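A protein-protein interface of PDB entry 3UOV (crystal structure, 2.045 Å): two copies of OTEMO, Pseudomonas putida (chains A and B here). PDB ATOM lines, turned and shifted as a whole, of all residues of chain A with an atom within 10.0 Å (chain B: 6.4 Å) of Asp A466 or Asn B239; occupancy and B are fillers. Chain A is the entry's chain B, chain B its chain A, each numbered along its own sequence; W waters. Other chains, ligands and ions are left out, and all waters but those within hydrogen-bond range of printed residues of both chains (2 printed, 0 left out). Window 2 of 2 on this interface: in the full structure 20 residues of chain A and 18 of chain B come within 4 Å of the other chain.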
ATOM      1  N   ASP A  11     -19.856  -1.113  15.190  1.00  0.00           N
ATOM      2  CA  ASP A  11     -18.865  -1.018  14.109  1.00  0.00           C
ATOM      3  C   ASP A  11     -17.576  -0.417  14.676  1.00  0.00           C
ATOM      4  O   ASP A  11     -16.480  -0.855  14.347  1.00  0.00           O
ATOM      5  CB  ASP A  11     -19.369  -0.174  12.929  1.00  0.00           C
ATOM      6  CG  ASP A  11     -20.498  -0.856  12.146  1.00  0.00           C
ATOM      7  OD1 ASP A  11     -20.281  -1.985  11.635  1.00  0.00           O
ATOM      8  OD2 ASP A  11     -21.591  -0.254  12.027  1.00  0.00           O
ATOM      9  N   ALA A  31     -22.023   8.047   7.979  1.00  0.00           N
ATOM     10  CA  ALA A  31     -21.866   7.017   6.961  1.00  0.00           C
ATOM     11  C   ALA A  31     -22.840   5.839   7.167  1.00  0.00           C
ATOM     12  O   ALA A  31     -22.901   4.921   6.350  1.00  0.00           O
ATOM     13  CB  ALA A  31     -20.425   6.525   6.939  1.00  0.00           C
ATOM     14  N   GLY A  32     -23.588   5.865   8.265  1.00  0.00           N
ATOM     15  CA  GLY A  32     -24.614   4.848   8.514  1.00  0.00           C
ATOM     16  C   GLY A  32     -24.035   3.650   9.230  1.00  0.00           C
ATOM     17  O   GLY A  32     -24.484   2.526   9.029  1.00  0.00           O
ATOM     18  N   MET A  33     -23.019   3.882  10.065  1.00  0.00           N
ATOM     19  CA  MET A  33     -22.455   2.819  10.873  1.00  0.00           C
ATOM     20  C   MET A  33     -22.686   3.104  12.350  1.00  0.00           C
ATOM     21  O   MET A  33     -22.952   4.249  12.733  1.00  0.00           O
ATOM     22  CB  MET A  33     -20.972   2.646  10.555  1.00  0.00           C
ATOM     23  CG  MET A  33     -20.713   1.862   9.271  1.00  0.00           C
ATOM     24  SD  MET A  33     -18.951   1.718   8.879  1.00  0.00           S
ATOM     25  CE  MET A  33     -18.636   3.301   8.117  1.00  0.00           C
ATOM     26  N   PHE A 138     -13.892  -2.143  15.131  1.00  0.00           N
ATOM     27  CA  PHE A 138     -12.745  -1.255  15.022  1.00  0.00           C
ATOM     28  C   PHE A 138     -12.613  -0.379  16.257  1.00  0.00           C
ATOM     29  O   PHE A 138     -13.599   0.180  16.738  1.00  0.00           O
ATOM     30  CB  PHE A 138     -12.882  -0.369  13.780  1.00  0.00           C
ATOM     31  CG  PHE A 138     -13.001  -1.137  12.488  1.00  0.00           C
ATOM     32  CD1 PHE A 138     -11.895  -1.750  11.917  1.00  0.00           C
ATOM     33  CD2 PHE A 138     -14.219  -1.224  11.827  1.00  0.00           C
ATOM     34  CE1 PHE A 138     -12.015  -2.475  10.717  1.00  0.00           C
ATOM     35  CE2 PHE A 138     -14.336  -1.927  10.626  1.00  0.00           C
ATOM     36  CZ  PHE A 138     -13.231  -2.556  10.086  1.00  0.00           C
ATOM     37  N   LEU A 458     -12.373   6.832   7.895  1.00  0.00           N
ATOM     38  CA  LEU A 458     -13.771   6.594   7.532  1.00  0.00           C
ATOM     39  C   LEU A 458     -13.855   5.931   6.145  1.00  0.00           C
ATOM     40  O   LEU A 458     -14.609   4.970   5.934  1.00  0.00           O
ATOM     41  CB  LEU A 458     -14.531   7.936   7.548  1.00  0.00           C
ATOM     42  CG  LEU A 458     -16.064   8.018   7.381  1.00  0.00           C
ATOM     43  CD1 LEU A 458     -16.499   8.313   5.969  1.00  0.00           C
ATOM     44  CD2 LEU A 458     -16.762   6.770   7.922  1.00  0.00           C
ATOM     45  N   ARG A 459     -13.088   6.446   5.191  1.00  0.00           N
ATOM     46  CA  ARG A 459     -13.052   5.835   3.854  1.00  0.00           C
ATOM     47  C   ARG A 459     -12.533   4.392   3.885  1.00  0.00           C
ATOM     48  O   ARG A 459     -13.081   3.521   3.215  1.00  0.00           O
ATOM     49  CB  ARG A 459     -12.262   6.705   2.877  1.00  0.00           C
ATOM     50  CG  ARG A 459     -12.999   7.972   2.466  1.00  0.00           C
ATOM     51  CD  ARG A 459     -12.301   8.685   1.305  1.00  0.00           C
ATOM     52  NE  ARG A 459     -10.983   9.211   1.641  1.00  0.00           N
ATOM     53  CZ  ARG A 459     -10.748  10.422   2.140  1.00  0.00           C
ATOM     54  NH1 ARG A 459      -9.508  10.816   2.373  1.00  0.00           N
ATOM     55  NH2 ARG A 459     -11.737  11.254   2.392  1.00  0.00           N
ATOM     56  N   MET A 460     -11.521   4.127   4.711  1.00  0.00           N
ATOM     57  CA  MET A 460     -11.046   2.761   4.884  1.00  0.00           C
ATOM     58  C   MET A 460     -12.101   1.873   5.549  1.00  0.00           C
ATOM     59  O   MET A 460     -12.331   0.747   5.119  1.00  0.00           O
ATOM     60  CB  MET A 460      -9.740   2.697   5.694  1.00  0.00           C
ATOM     61  CG  MET A 460      -9.198   1.269   5.810  1.00  0.00           C
ATOM     62  SD  MET A 460      -7.493   1.228   6.367  1.00  0.00           S
ATOM     63  CE  MET A 460      -7.201  -0.528   6.507  1.00  0.00           C
ATOM     64  N   ILE A 461     -12.702   2.359   6.624  1.00  0.00           N
ATOM     65  CA  ILE A 461     -13.762   1.588   7.260  1.00  0.00           C
ATOM     66  C   ILE A 461     -14.935   1.337   6.300  1.00  0.00           C
ATOM     67  O   ILE A 461     -15.433   0.213   6.230  1.00  0.00           O
ATOM     68  CB  ILE A 461     -14.197   2.168   8.622  1.00  0.00           C
ATOM     69  CG1 ILE A 461     -13.058   1.999   9.637  1.00  0.00           C
ATOM     70  CG2 ILE A 461     -15.408   1.412   9.163  1.00  0.00           C
ATOM     71  CD1 ILE A 461     -13.238   2.868  10.889  1.00  0.00           C
ATOM     72  N   SER A 462     -15.331   2.340   5.523  1.00  0.00           N
ATOM     73  CA  SER A 462     -16.420   2.151   4.561  1.00  0.00           C
ATOM     74  C   SER A 462     -16.074   1.157   3.456  1.00  0.00           C
ATOM     75  O   SER A 462     -16.930   0.394   3.042  1.00  0.00           O
ATOM     76  CB  SER A 462     -16.911   3.471   3.974  1.00  0.00           C
ATOM     77  OG  SER A 462     -17.333   4.335   5.014  1.00  0.00           O
ATOM     78  N   TYR A 463     -14.816   1.144   3.017  1.00  0.00           N
ATOM     79  CA  TYR A 463     -14.336   0.181   2.018  1.00  0.00           C
ATOM     80  C   TYR A 463     -14.431  -1.244   2.562  1.00  0.00           C
ATOM     81  O   TYR A 463     -14.894  -2.161   1.876  1.00  0.00           O
ATOM     82  CB  TYR A 463     -12.893   0.510   1.641  1.00  0.00           C
ATOM     83  CG  TYR A 463     -12.198  -0.479   0.719  1.00  0.00           C
ATOM     84  CD1 TYR A 463     -12.239  -0.317  -0.667  1.00  0.00           C
ATOM     85  CD2 TYR A 463     -11.474  -1.549   1.234  1.00  0.00           C
ATOM     86  CE1 TYR A 463     -11.588  -1.215  -1.519  1.00  0.00           C
ATOM     87  CE2 TYR A 463     -10.824  -2.455   0.397  1.00  0.00           C
ATOM     88  CZ  TYR A 463     -10.887  -2.278  -0.980  1.00  0.00           C
ATOM     89  OH  TYR A 463     -10.228  -3.164  -1.807  1.00  0.00           O
ATOM     90  N   MET A 464     -13.984  -1.424   3.800  1.00  0.00           N
ATOM     91  CA  MET A 464     -14.083  -2.710   4.467  1.00  0.00           C
ATOM     92  C   MET A 464     -15.537  -3.178   4.583  1.00  0.00           C
ATOM     93  O   MET A 464     -15.859  -4.297   4.209  1.00  0.00           O
ATOM     94  CB  MET A 464     -13.352  -2.668   5.822  1.00  0.00           C
ATOM     95  CG  MET A 464     -11.829  -2.596   5.631  1.00  0.00           C
ATOM     96  SD  MET A 464     -10.914  -2.674   7.158  1.00  0.00           S
ATOM     97  CE  MET A 464     -11.099  -4.390   7.583  1.00  0.00           C
ATOM     98  N   LYS A 465     -16.412  -2.308   5.064  1.00  0.00           N
ATOM     99  CA  LYS A 465     -17.836  -2.644   5.150  1.00  0.00           C
ATOM    100  C   LYS A 465     -18.387  -3.016   3.768  1.00  0.00           C
ATOM    101  O   LYS A 465     -19.036  -4.047   3.617  1.00  0.00           O
ATOM    102  CB  LYS A 465     -18.655  -1.501   5.770  1.00  0.00           C
ATOM    103  CG  LYS A 465     -20.117  -1.884   5.996  1.00  0.00           C
ATOM    104  CD  LYS A 465     -21.008  -0.756   6.539  1.00  0.00           C
ATOM    105  CE  LYS A 465     -22.481  -1.238   6.552  1.00  0.00           C
ATOM    106  NZ  LYS A 465     -23.420  -0.270   7.199  1.00  0.00           N
ATOM    107  N   ASP A 466     -18.096  -2.192   2.762  1.00  0.00           N
ATOM    108  CA  ASP A 466     -18.531  -2.474   1.388  1.00  0.00           C
ATOM    109  C   ASP A 466     -18.089  -3.844   0.847  1.00  0.00           C
ATOM    110  O   ASP A 466     -18.821  -4.483   0.083  1.00  0.00           O
ATOM    111  CB  ASP A 466     -18.064  -1.368   0.446  1.00  0.00           C
ATOM    112  CG  ASP A 466     -18.845  -0.067   0.627  1.00  0.00           C
ATOM    113  OD1 ASP A 466     -19.897  -0.074   1.301  1.00  0.00           O
ATOM    114  OD2 ASP A 466     -18.407   0.967   0.087  1.00  0.00           O
ATOM    115  N   ASN A 467     -16.887  -4.279   1.225  1.00  0.00           N
ATOM    116  CA  ASN A 467     -16.324  -5.512   0.701  1.00  0.00           C
ATOM    117  C   ASN A 467     -16.469  -6.687   1.647  1.00  0.00           C
ATOM    118  O   ASN A 467     -16.021  -7.782   1.338  1.00  0.00           O
ATOM    119  CB  ASN A 467     -14.852  -5.322   0.356  1.00  0.00           C
ATOM    120  CG  ASN A 467     -14.644  -4.388  -0.806  1.00  0.00           C
ATOM    121  OD1 ASN A 467     -14.351  -3.205  -0.622  1.00  0.00           O
ATOM    122  ND2 ASN A 467     -14.812  -4.901  -2.010  1.00  0.00           N
ATOM    123  N   GLY A 468     -17.077  -6.451   2.800  1.00  0.00           N
ATOM    124  CA  GLY A 468     -17.286  -7.492   3.797  1.00  0.00           C
ATOM    125  C   GLY A 468     -16.034  -7.910   4.536  1.00  0.00           C
ATOM    126  O   GLY A 468     -16.028  -8.966   5.156  1.00  0.00           O
ATOM    127  N   PHE A 469     -14.974  -7.098   4.479  1.00  0.00           N
ATOM    128  CA  PHE A 469     -13.755  -7.348   5.265  1.00  0.00           C
ATOM    129  C   PHE A 469     -13.936  -6.956   6.730  1.00  0.00           C
ATOM    130  O   PHE A 469     -14.468  -5.883   7.018  1.00  0.00           O
ATOM    131  CB  PHE A 469     -12.553  -6.557   4.722  1.00  0.00           C
ATOM    132  CG  PHE A 469     -12.212  -6.847   3.297  1.00  0.00           C
ATOM    133  CD1 PHE A 469     -12.153  -8.165   2.825  1.00  0.00           C
ATOM    134  CD2 PHE A 469     -11.912  -5.806   2.426  1.00  0.00           C
ATOM    135  CE1 PHE A 469     -11.829  -8.426   1.492  1.00  0.00           C
ATOM    136  CE2 PHE A 469     -11.591  -6.056   1.098  1.00  0.00           C
ATOM    137  CZ  PHE A 469     -11.543  -7.367   0.629  1.00  0.00           C
ATOM    138  N   THR A 470     -13.451  -7.814   7.634  1.00  0.00           N
ATOM    139  CA  THR A 470     -13.568  -7.635   9.076  1.00  0.00           C
ATOM    140  C   THR A 470     -12.196  -7.661   9.768  1.00  0.00           C
ATOM    141  O   THR A 470     -12.097  -7.643  10.991  1.00  0.00           O
ATOM    142  CB  THR A 470     -14.418  -8.759   9.697  1.00  0.00           C
ATOM    143  OG1 THR A 470     -13.946 -10.014   9.210  1.00  0.00           O
ATOM    144  CG2 THR A 470     -15.912  -8.609   9.335  1.00  0.00           C
ATOM    145  N   TYR A 539      -5.642  -0.742  -0.451  1.00  0.00           N
ATOM    146  CA  TYR A 539      -5.007  -0.681   0.859  1.00  0.00           C
ATOM    147  C   TYR A 539      -3.784  -1.579   0.932  1.00  0.00           C
ATOM    148  O   TYR A 539      -3.536  -2.198   1.943  1.00  0.00           O
ATOM    149  CB  TYR A 539      -6.022  -0.941   1.992  1.00  0.00           C
ATOM    150  CG  TYR A 539      -7.051   0.173   2.026  1.00  0.00           C
ATOM    151  CD1 TYR A 539      -8.198   0.104   1.238  1.00  0.00           C
ATOM    152  CD2 TYR A 539      -6.832   1.327   2.775  1.00  0.00           C
ATOM    153  CE1 TYR A 539      -9.139   1.150   1.221  1.00  0.00           C
ATOM    154  CE2 TYR A 539      -7.750   2.376   2.753  1.00  0.00           C
ATOM    155  CZ  TYR A 539      -8.908   2.276   1.974  1.00  0.00           C
ATOM    156  OH  TYR A 539      -9.844   3.293   1.942  1.00  0.00           O
ATOM    157  N   MET B 234     -18.462  -1.817 -11.896  1.00  0.00           N
ATOM    158  CA  MET B 234     -18.951  -0.452 -11.978  1.00  0.00           C
ATOM    159  C   MET B 234     -19.463  -0.035 -10.611  1.00  0.00           C
ATOM    160  O   MET B 234     -19.174   1.064 -10.156  1.00  0.00           O
ATOM    161  CB  MET B 234     -20.042  -0.322 -13.049  1.00  0.00           C
ATOM    162  CG  MET B 234     -20.431   1.121 -13.440  1.00  0.00           C
ATOM    163  SD  MET B 234     -19.066   2.230 -13.897  1.00  0.00           S
ATOM    164  CE  MET B 234     -19.129   3.447 -12.590  1.00  0.00           C
ATOM    165  N   ASP B 235     -20.182  -0.939  -9.946  1.00  0.00           N
ATOM    166  CA  ASP B 235     -20.712  -0.677  -8.608  1.00  0.00           C
ATOM    167  C   ASP B 235     -19.614  -0.469  -7.578  1.00  0.00           C
ATOM    168  O   ASP B 235     -19.687   0.465  -6.776  1.00  0.00           O
ATOM    169  CB  ASP B 235     -21.646  -1.798  -8.157  1.00  0.00           C
ATOM    170  CG  ASP B 235     -22.989  -1.770  -8.869  1.00  0.00           C
ATOM    171  OD1 ASP B 235     -23.317  -0.750  -9.514  1.00  0.00           O
ATOM    172  OD2 ASP B 235     -23.728  -2.772  -8.784  1.00  0.00           O
ATOM    173  N   SER B 236     -18.600  -1.334  -7.578  1.00  0.00           N
ATOM    174  CA  SER B 236     -17.540  -1.213  -6.579  1.00  0.00           C
ATOM    175  C   SER B 236     -16.702   0.047  -6.824  1.00  0.00           C
ATOM    176  O   SER B 236     -16.282   0.707  -5.864  1.00  0.00           O
ATOM    177  CB  SER B 236     -16.675  -2.471  -6.489  1.00  0.00           C
ATOM    178  OG  SER B 236     -15.671  -2.480  -7.477  1.00  0.00           O
ATOM    179  N   LEU B 237     -16.489   0.382  -8.101  1.00  0.00           N
ATOM    180  CA  LEU B 237     -15.912   1.688  -8.478  1.00  0.00           C
ATOM    181  C   LEU B 237     -16.693   2.845  -7.864  1.00  0.00           C
ATOM    182  O   LEU B 237     -16.143   3.633  -7.100  1.00  0.00           O
ATOM    183  CB  LEU B 237     -15.835   1.846 -10.001  1.00  0.00           C
ATOM    184  CG  LEU B 237     -14.688   1.080 -10.664  1.00  0.00           C
ATOM    185  CD1 LEU B 237     -14.817   1.094 -12.181  1.00  0.00           C
ATOM    186  CD2 LEU B 237     -13.329   1.645 -10.220  1.00  0.00           C
ATOM    187  N   ARG B 238     -17.986   2.930  -8.164  1.00  0.00           N
ATOM    188  CA  ARG B 238     -18.813   3.989  -7.610  1.00  0.00           C
ATOM    189  C   ARG B 238     -18.765   4.066  -6.069  1.00  0.00           C
ATOM    190  O   ARG B 238     -18.759   5.158  -5.522  1.00  0.00           O
ATOM    191  CB  ARG B 238     -20.256   3.856  -8.102  1.00  0.00           C
ATOM    192  CG  ARG B 238     -21.187   4.990  -7.670  1.00  0.00           C
ATOM    193  CD  ARG B 238     -22.622   4.779  -8.211  1.00  0.00           C
ATOM    194  NE  ARG B 238     -22.605   4.381  -9.616  1.00  0.00           N
ATOM    195  CZ  ARG B 238     -22.941   3.175 -10.068  1.00  0.00           C
ATOM    196  NH1 ARG B 238     -23.338   2.222  -9.235  1.00  0.00           N
ATOM    197  NH2 ARG B 238     -22.874   2.918 -11.368  1.00  0.00           N
ATOM    198  N   ASN B 239     -18.722   2.921  -5.388  1.00  0.00           N
ATOM    199  CA  ASN B 239     -18.624   2.899  -3.925  1.00  0.00           C
ATOM    200  C   ASN B 239     -17.298   3.517  -3.483  1.00  0.00           C
ATOM    201  O   ASN B 239     -17.222   4.114  -2.423  1.00  0.00           O
ATOM    202  CB  ASN B 239     -18.721   1.474  -3.388  1.00  0.00           C
ATOM    203  CG  ASN B 239     -20.156   0.939  -3.369  1.00  0.00           C
ATOM    204  OD1 ASN B 239     -21.119   1.703  -3.355  1.00  0.00           O
ATOM    205  ND2 ASN B 239     -20.294  -0.395  -3.361  1.00  0.00           N
ATOM    206  N   ARG B 240     -16.288   3.394  -4.346  1.00  0.00           N
ATOM    207  CA  ARG B 240     -14.915   3.866  -4.107  1.00  0.00           C
ATOM    208  C   ARG B 240     -14.650   5.288  -4.601  1.00  0.00           C
ATOM    209  O   ARG B 240     -13.516   5.768  -4.526  1.00  0.00           O
ATOM    210  CB  ARG B 240     -13.940   2.919  -4.818  1.00  0.00           C
ATOM    211  CG  ARG B 240     -13.154   2.053  -3.891  1.00  0.00           C
ATOM    212  CD  ARG B 240     -12.662   0.764  -4.526  1.00  0.00           C
ATOM    213  NE  ARG B 240     -11.998   0.885  -5.823  1.00  0.00           N
ATOM    214  CZ  ARG B 240     -10.719   1.210  -6.016  1.00  0.00           C
ATOM    215  NH1 ARG B 240     -10.236   1.244  -7.245  1.00  0.00           N
ATOM    216  NH2 ARG B 240      -9.923   1.514  -5.009  1.00  0.00           N
ATOM    217  N   TYR B 241     -15.678   5.961  -5.109  1.00  0.00           N
ATOM    218  CA  TYR B 241     -15.492   7.272  -5.730  1.00  0.00           C
ATOM    219  C   TYR B 241     -14.763   8.285  -4.830  1.00  0.00           C
ATOM    220  O   TYR B 241     -13.849   8.965  -5.316  1.00  0.00           O
ATOM    221  CB  TYR B 241     -16.822   7.864  -6.243  1.00  0.00           C
ATOM    222  CG  TYR B 241     -17.201   7.483  -7.668  1.00  0.00           C
ATOM    223  CD1 TYR B 241     -16.363   6.689  -8.466  1.00  0.00           C
ATOM    224  CD2 TYR B 241     -18.386   7.961  -8.231  1.00  0.00           C
ATOM    225  CE1 TYR B 241     -16.714   6.358  -9.764  1.00  0.00           C
ATOM    226  CE2 TYR B 241     -18.738   7.653  -9.548  1.00  0.00           C
ATOM    227  CZ  TYR B 241     -17.906   6.852 -10.303  1.00  0.00           C
ATOM    228  OH  TYR B 241     -18.266   6.554 -11.602  1.00  0.00           O
ATOM    229  N   PRO B 242     -15.145   8.386  -3.525  1.00  0.00           N
ATOM    230  CA  PRO B 242     -14.435   9.337  -2.636  1.00  0.00           C
ATOM    231  C   PRO B 242     -12.915   9.156  -2.560  1.00  0.00           C
ATOM    232  O   PRO B 242     -12.191  10.142  -2.543  1.00  0.00           O
ATOM    233  CB  PRO B 242     -15.103   9.117  -1.274  1.00  0.00           C
ATOM    234  CG  PRO B 242     -16.504   8.657  -1.639  1.00  0.00           C
ATOM    235  CD  PRO B 242     -16.243   7.715  -2.796  1.00  0.00           C
ATOM    236  N   THR B 243     -12.450   7.913  -2.529  1.00  0.00           N
ATOM    237  CA  THR B 243     -11.030   7.593  -2.569  1.00  0.00           C
ATOM    238  C   THR B 243     -10.457   7.863  -3.957  1.00  0.00           C
ATOM    239  O   THR B 243      -9.361   8.423  -4.072  1.00  0.00           O
ATOM    240  CB  THR B 243     -10.790   6.117  -2.205  1.00  0.00           C
ATOM    241  OG1 THR B 243     -11.050   5.929  -0.810  1.00  0.00           O
ATOM    242  CG2 THR B 243      -9.346   5.702  -2.517  1.00  0.00           C
HETATM  243  O   HOH W   1     -11.520   3.394  -0.299  1.00  0.00           O
HETATM  244  O   HOH W   2      -9.028   7.181   0.926  1.00  0.00           O
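Printed residues of chain B within 4 Å of Arg A459: Pro B242 and Thr B243. Printed residues of chain B within 4 Å of Tyr A463: Arg B240. Gly A468 touches none of the printed residues of chain B. Printed residues of chain B within 4 Å of Tyr A539: Thr B243. Leu B237 touches none of the printed residues of chain A. Asn B239 touches one residue of chain A. Printed residues of chain A within 4 Å of Arg B240: Tyr A463 (3.8 Å). The nearest residue of chain B that does not touch Asp A466 is Arg B240 (5.5 Å). The nearest printed residue of chain B that does not touch Arg A459 is Tyr B241 (6.6 Å).
No position is printed for both chains. Of the 5 pairs that touch across the chains among the printed residues, none has its exchanged pair printed and touching as well.
Water W1 bridges OG1 of Thr B243 (2.6 Å) and OH of Tyr A539 (2.8 Å). Water W2 bridges NE of Arg A459 (2.9 Å) and OG1 of Thr B243 (2.9 Å).
Among the printed residues, merely in contact across the chains: Arg A459 with Pro B242 (3.8 Å), Arg A459 with Thr B243 (3.7 Å), Tyr A463 with Arg B240 (3.8 Å), Asp A466 with Asn B239 (3.5 Å) and Tyr A539 with Thr B243 (3.997 Å).
Among the printed residues, no Asp or Glu carboxylate lies within 4 Å of a Lys or Arg side-chain nitrogen of the other chain.
The backbone carbonyl oxygen (O) of Tyr A463 lies close to the side-chain amide oxygen (OD1) of Asn A467 (2.8 Å). OH of Tyr A539 is in hydrogen-bond range of O of Arg A459, at 3.5 Å. The backbone NH of Met A460 lies close to the side-chain hydroxyl of Tyr A539 (3.3 Å).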
